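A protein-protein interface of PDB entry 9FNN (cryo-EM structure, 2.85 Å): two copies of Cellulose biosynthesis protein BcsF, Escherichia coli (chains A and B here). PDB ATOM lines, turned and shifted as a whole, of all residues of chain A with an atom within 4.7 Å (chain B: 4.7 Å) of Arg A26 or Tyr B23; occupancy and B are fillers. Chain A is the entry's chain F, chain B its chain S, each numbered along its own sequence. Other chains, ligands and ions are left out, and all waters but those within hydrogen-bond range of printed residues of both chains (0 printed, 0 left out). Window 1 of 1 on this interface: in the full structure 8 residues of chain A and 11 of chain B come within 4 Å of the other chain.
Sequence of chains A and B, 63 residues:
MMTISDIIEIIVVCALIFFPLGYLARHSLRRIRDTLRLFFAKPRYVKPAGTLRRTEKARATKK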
ATOM      1  N   GLY A  22      15.854  17.618 -12.603  1.00  0.00           N
ATOM      2  CA  GLY A  22      15.205  16.719 -13.574  1.00  0.00           C
ATOM      3  C   GLY A  22      13.791  16.367 -13.146  1.00  0.00           C
ATOM      4  O   GLY A  22      12.981  16.046 -14.036  1.00  0.00           O
ATOM      5  N   TYR A  23      13.493  16.430 -11.841  1.00  0.00           N
ATOM      6  CA  TYR A  23      12.118  16.180 -11.420  1.00  0.00           C
ATOM      7  C   TYR A  23      11.209  17.341 -11.802  1.00  0.00           C
ATOM      8  O   TYR A  23      10.094  17.132 -12.294  1.00  0.00           O
ATOM      9  CB  TYR A  23      12.077  15.933  -9.913  1.00  0.00           C
ATOM     10  CG  TYR A  23      10.915  15.086  -9.450  1.00  0.00           C
ATOM     11  CD1 TYR A  23      10.923  13.710  -9.624  1.00  0.00           C
ATOM     12  CD2 TYR A  23       9.817  15.660  -8.825  1.00  0.00           C
ATOM     13  CE1 TYR A  23       9.869  12.929  -9.196  1.00  0.00           C
ATOM     14  CE2 TYR A  23       8.756  14.888  -8.393  1.00  0.00           C
ATOM     15  CZ  TYR A  23       8.787  13.523  -8.582  1.00  0.00           C
ATOM     16  OH  TYR A  23       7.732  12.750  -8.155  1.00  0.00           O
ATOM     17  N   LEU A  24      11.675  18.573 -11.590  1.00  0.00           N
ATOM     18  CA  LEU A  24      10.891  19.742 -11.976  1.00  0.00           C
ATOM     19  C   LEU A  24      10.717  19.813 -13.487  1.00  0.00           C
ATOM     20  O   LEU A  24       9.647  20.194 -13.977  1.00  0.00           O
ATOM     21  CB  LEU A  24      11.552  21.018 -11.452  1.00  0.00           C
ATOM     22  CG  LEU A  24      11.024  21.586 -10.131  1.00  0.00           C
ATOM     23  CD1 LEU A  24       9.562  21.982 -10.267  1.00  0.00           C
ATOM     24  CD2 LEU A  24      11.210  20.598  -8.990  1.00  0.00           C
ATOM     25  N   ALA A  25      11.759  19.461 -14.242  1.00  0.00           N
ATOM     26  CA  ALA A  25      11.647  19.455 -15.695  1.00  0.00           C
ATOM     27  C   ALA A  25      10.605  18.446 -16.158  1.00  0.00           C
ATOM     28  O   ALA A  25       9.825  18.721 -17.077  1.00  0.00           O
ATOM     29  CB  ALA A  25      13.005  19.157 -16.328  1.00  0.00           C
ATOM     30  N   ARG A  26      10.581  17.267 -15.534  1.00  0.00           N
ATOM     31  CA  ARG A  26       9.566  16.275 -15.873  1.00  0.00           C
ATOM     32  C   ARG A  26       8.170  16.754 -15.499  1.00  0.00           C
ATOM     33  O   ARG A  26       7.212  16.535 -16.250  1.00  0.00           O
ATOM     34  CB  ARG A  26       9.876  14.949 -15.188  1.00  0.00           C
ATOM     35  CG  ARG A  26      10.405  13.893 -16.128  1.00  0.00           C
ATOM     36  CD  ARG A  26       9.388  13.565 -17.208  1.00  0.00           C
ATOM     37  NE  ARG A  26       8.311  12.715 -16.717  1.00  0.00           N
ATOM     38  CZ  ARG A  26       7.068  13.125 -16.512  1.00  0.00           C
ATOM     39  NH1 ARG A  26       6.702  14.370 -16.762  1.00  0.00           N
ATOM     40  NH2 ARG A  26       6.168  12.264 -16.048  1.00  0.00           N
ATOM     41  N   HIS A  27       8.030  17.404 -14.340  1.00  0.00           N
ATOM     42  CA  HIS A  27       6.716  17.881 -13.919  1.00  0.00           C
ATOM     43  C   HIS A  27       6.135  18.876 -14.910  1.00  0.00           C
ATOM     44  O   HIS A  27       4.912  19.027 -14.992  1.00  0.00           O
ATOM     45  CB  HIS A  27       6.803  18.514 -12.531  1.00  0.00           C
ATOM     46  CG  HIS A  27       6.352  17.613 -11.424  1.00  0.00           C
ATOM     47  ND1 HIS A  27       5.042  17.553 -11.002  1.00  0.00           N
ATOM     48  CD2 HIS A  27       7.038  16.740 -10.649  1.00  0.00           C
ATOM     49  CE1 HIS A  27       4.939  16.680 -10.016  1.00  0.00           C
ATOM     50  NE2 HIS A  27       6.136  16.173  -9.783  1.00  0.00           N
ATOM     51  N   SER A  28       7.024  19.619 -15.559  1.00  0.00           N
ATOM     52  CA  SER A  28       6.563  20.602 -16.561  1.00  0.00           C
ATOM     53  C   SER A  28       6.571  19.926 -17.930  1.00  0.00           C
ATOM     54  O   SER A  28       6.749  20.641 -18.910  1.00  0.00           O
ATOM     55  CB  SER A  28       7.423  21.839 -16.543  1.00  0.00           C
ATOM     56  OG  SER A  28       8.790  21.512 -16.740  1.00  0.00           O
ATOM     57  N   LEU A  29       6.362  18.609 -18.005  1.00  0.00           N
ATOM     58  CA  LEU A  29       6.294  17.932 -19.329  1.00  0.00           C
ATOM     59  C   LEU A  29       5.284  18.648 -20.232  1.00  0.00           C
ATOM     60  O   LEU A  29       5.678  19.044 -21.342  1.00  0.00           O
ATOM     61  CB  LEU A  29       5.906  16.462 -19.151  1.00  0.00           C
ATOM     62  CG  LEU A  29       5.734  15.675 -20.449  1.00  0.00           C
ATOM     63  CD1 LEU A  29       7.042  15.603 -21.221  1.00  0.00           C
ATOM     64  CD2 LEU A  29       5.200  14.278 -20.171  1.00  0.00           C
ATOM     65  N   PHE B  19      20.219  12.938 -15.110  1.00  0.00           N
ATOM     66  CA  PHE B  19      19.011  13.454 -15.812  1.00  0.00           C
ATOM     67  C   PHE B  19      18.002  12.303 -15.949  1.00  0.00           C
ATOM     68  O   PHE B  19      16.917  12.470 -15.381  1.00  0.00           O
ATOM     69  CB  PHE B  19      19.372  14.182 -17.112  1.00  0.00           C
ATOM     70  CG  PHE B  19      18.441  15.318 -17.452  1.00  0.00           C
ATOM     71  CD1 PHE B  19      18.108  16.268 -16.500  1.00  0.00           C
ATOM     72  CD2 PHE B  19      17.885  15.428 -18.716  1.00  0.00           C
ATOM     73  CE1 PHE B  19      17.247  17.311 -16.808  1.00  0.00           C
ATOM     74  CE2 PHE B  19      17.025  16.471 -19.024  1.00  0.00           C
ATOM     75  CZ  PHE B  19      16.707  17.409 -18.069  1.00  0.00           C
ATOM     76  N   PRO B  20      18.265  11.170 -16.654  1.00  0.00           N
ATOM     77  CA  PRO B  20      17.341  10.022 -16.667  1.00  0.00           C
ATOM     78  C   PRO B  20      17.110   9.463 -15.257  1.00  0.00           C
ATOM     79  O   PRO B  20      16.029   8.956 -15.017  1.00  0.00           O
ATOM     80  CB  PRO B  20      18.045   8.960 -17.520  1.00  0.00           C
ATOM     81  CG  PRO B  20      18.903   9.769 -18.451  1.00  0.00           C
ATOM     82  CD  PRO B  20      19.363  10.927 -17.592  1.00  0.00           C
ATOM     83  N   LEU B  21      18.112   9.556 -14.373  1.00  0.00           N
ATOM     84  CA  LEU B  21      17.910   9.118 -12.966  1.00  0.00           C
ATOM     85  C   LEU B  21      16.724   9.895 -12.391  1.00  0.00           C
ATOM     86  O   LEU B  21      15.875   9.263 -11.740  1.00  0.00           O
ATOM     87  CB  LEU B  21      19.184   9.380 -12.157  1.00  0.00           C
ATOM     88  CG  LEU B  21      19.112   9.047 -10.667  1.00  0.00           C
ATOM     89  CD1 LEU B  21      18.872   7.562 -10.444  1.00  0.00           C
ATOM     90  CD2 LEU B  21      20.377   9.495  -9.953  1.00  0.00           C
ATOM     91  N   GLY B  22      16.673  11.211 -12.631  1.00  0.00           N
ATOM     92  CA  GLY B  22      15.537  12.033 -12.169  1.00  0.00           C
ATOM     93  C   GLY B  22      14.391  12.034 -13.169  1.00  0.00           C
ATOM     94  O   GLY B  22      13.275  12.429 -12.776  1.00  0.00           O
ATOM     95  N   TYR B  23      14.647  11.609 -14.414  1.00  0.00           N
ATOM     96  CA  TYR B  23      13.568  11.533 -15.435  1.00  0.00           C
ATOM     97  C   TYR B  23      12.827  10.203 -15.274  1.00  0.00           C
ATOM     98  O   TYR B  23      11.588  10.207 -15.361  1.00  0.00           O
ATOM     99  CB  TYR B  23      14.137  11.731 -16.843  1.00  0.00           C
ATOM    100  CG  TYR B  23      13.117  11.572 -17.939  1.00  0.00           C
ATOM    101  CD1 TYR B  23      12.203  12.575 -18.218  1.00  0.00           C
ATOM    102  CD2 TYR B  23      13.075  10.424 -18.713  1.00  0.00           C
ATOM    103  CE1 TYR B  23      11.268  12.439 -19.230  1.00  0.00           C
ATOM    104  CE2 TYR B  23      12.149  10.273 -19.731  1.00  0.00           C
ATOM    105  CZ  TYR B  23      11.241  11.283 -19.990  1.00  0.00           C
ATOM    106  OH  TYR B  23      10.323  11.141 -20.990  1.00  0.00           O
ATOM    107  N   LEU B  24      13.558   9.110 -15.042  1.00  0.00           N
ATOM    108  CA  LEU B  24      12.953   7.801 -14.826  1.00  0.00           C
ATOM    109  C   LEU B  24      12.320   7.697 -13.447  1.00  0.00           C
ATOM    110  O   LEU B  24      11.341   6.964 -13.272  1.00  0.00           O
ATOM    111  CB  LEU B  24      13.991   6.695 -15.020  1.00  0.00           C
ATOM    112  CG  LEU B  24      14.108   6.092 -16.423  1.00  0.00           C
ATOM    113  CD1 LEU B  24      12.774   5.515 -16.869  1.00  0.00           C
ATOM    114  CD2 LEU B  24      14.617   7.112 -17.431  1.00  0.00           C
ATOM    115  N   ALA B  25      12.864   8.406 -12.458  1.00  0.00           N
ATOM    116  CA  ALA B  25      12.232   8.429 -11.145  1.00  0.00           C
ATOM    117  C   ALA B  25      10.847   9.056 -11.216  1.00  0.00           C
ATOM    118  O   ALA B  25       9.898   8.558 -10.599  1.00  0.00           O
ATOM    119  CB  ALA B  25      13.115   9.180 -10.149  1.00  0.00           C
ATOM    120  N   ARG B  26      10.710  10.152 -11.962  1.00  0.00           N
ATOM    121  CA  ARG B  26       9.401  10.785 -12.088  1.00  0.00           C
ATOM    122  C   ARG B  26       8.470   9.964 -12.971  1.00  0.00           C
ATOM    123  O   ARG B  26       7.267   9.875 -12.698  1.00  0.00           O
ATOM    124  CB  ARG B  26       9.542  12.203 -12.638  1.00  0.00           C
ATOM    125  CG  ARG B  26       8.210  12.882 -12.925  1.00  0.00           C
ATOM    126  CD  ARG B  26       7.336  12.949 -11.687  1.00  0.00           C
ATOM    127  NE  ARG B  26       6.007  13.470 -11.986  1.00  0.00           N
ATOM    128  CZ  ARG B  26       5.013  13.530 -11.111  1.00  0.00           C
ATOM    129  NH1 ARG B  26       5.162  13.112  -9.865  1.00  0.00           N
ATOM    130  NH2 ARG B  26       3.839  14.024 -11.496  1.00  0.00           N
ATOM    131  N   HIS B  27       9.003   9.359 -14.033  1.00  0.00           N
ATOM    132  CA  HIS B  27       8.154   8.621 -14.961  1.00  0.00           C
ATOM    133  C   HIS B  27       7.488   7.433 -14.279  1.00  0.00           C
ATOM    134  O   HIS B  27       6.317   7.134 -14.542  1.00  0.00           O
ATOM    135  CB  HIS B  27       8.973   8.157 -16.164  1.00  0.00           C
ATOM    136  CG  HIS B  27       8.141   7.726 -17.329  1.00  0.00           C
ATOM    137  ND1 HIS B  27       6.789   7.983 -17.412  1.00  0.00           N
ATOM    138  CD2 HIS B  27       8.467   7.058 -18.461  1.00  0.00           C
ATOM    139  CE1 HIS B  27       6.319   7.492 -18.545  1.00  0.00           C
ATOM    140  NE2 HIS B  27       7.317   6.925 -19.199  1.00  0.00           N
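CE1 of Phe B19 touches CA of Gly A22 (3.9 Å). Gly B22 touches Gly A22 (O to O, 3.8 Å). Tyr B23 touches Arg A26 (CE1 to CD, 3.0 Å). Arg A26 touches Arg B26.
Printed residues of chain B within 4 Å of Gly A22: Phe B19 (3.9 Å) and Gly B22 (3.8 Å). Of the printed residues of chain B, Tyr A23 touches Arg B26. Arg A26 touches two residues of chain B. Of chain A, only Arg A26 comes within 4 Å of Tyr B23. Printed residues of chain A within 4 Å of Arg B26: Tyr A23 (3.1 Å), Arg A26 (3.5 Å) and His A27 (3.2 Å). The nearest residue of chain B that does not touch Arg A26 is His B27 (4.3 Å). The nearest printed residue of chain A that does not touch Tyr B23 is Gly A22 (4.8 Å). The nearest printed residue of chain A that does not touch Arg B26 is Gly A22 (5.3 Å).
Printed residues of chain B that touch a printed residue of chain A: Phe B19, Gly B22, Tyr B23 and Arg B26. Hydrophobic or aromatic side chains of chain A that line the printed part of chain B: Tyr A23 and His A27. Among the printed residues, 6 pairs touch across the chains.
Gly A22 touches its own counterpart, Gly B22. Tyr A23 touches Arg B26, and with the chains exchanged Arg A26 touches Tyr B23. Arg B26 touches its own counterpart, Arg A26. His A27 touches Arg B26, but with the chains exchanged Arg A26 does not touch His B27 (4.3 Å). Of the 6 pairs that touch across the chains among the printed residues, 4 have their exchanged pair printed and touching as well.
A ring nitrogen (NE2) of His A27 lies close to the guanidinium group (NH1) of Arg B26. NH1 of Arg B26 lies within hydrogen-bond range of OH of Tyr A23 (3.1 Å).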
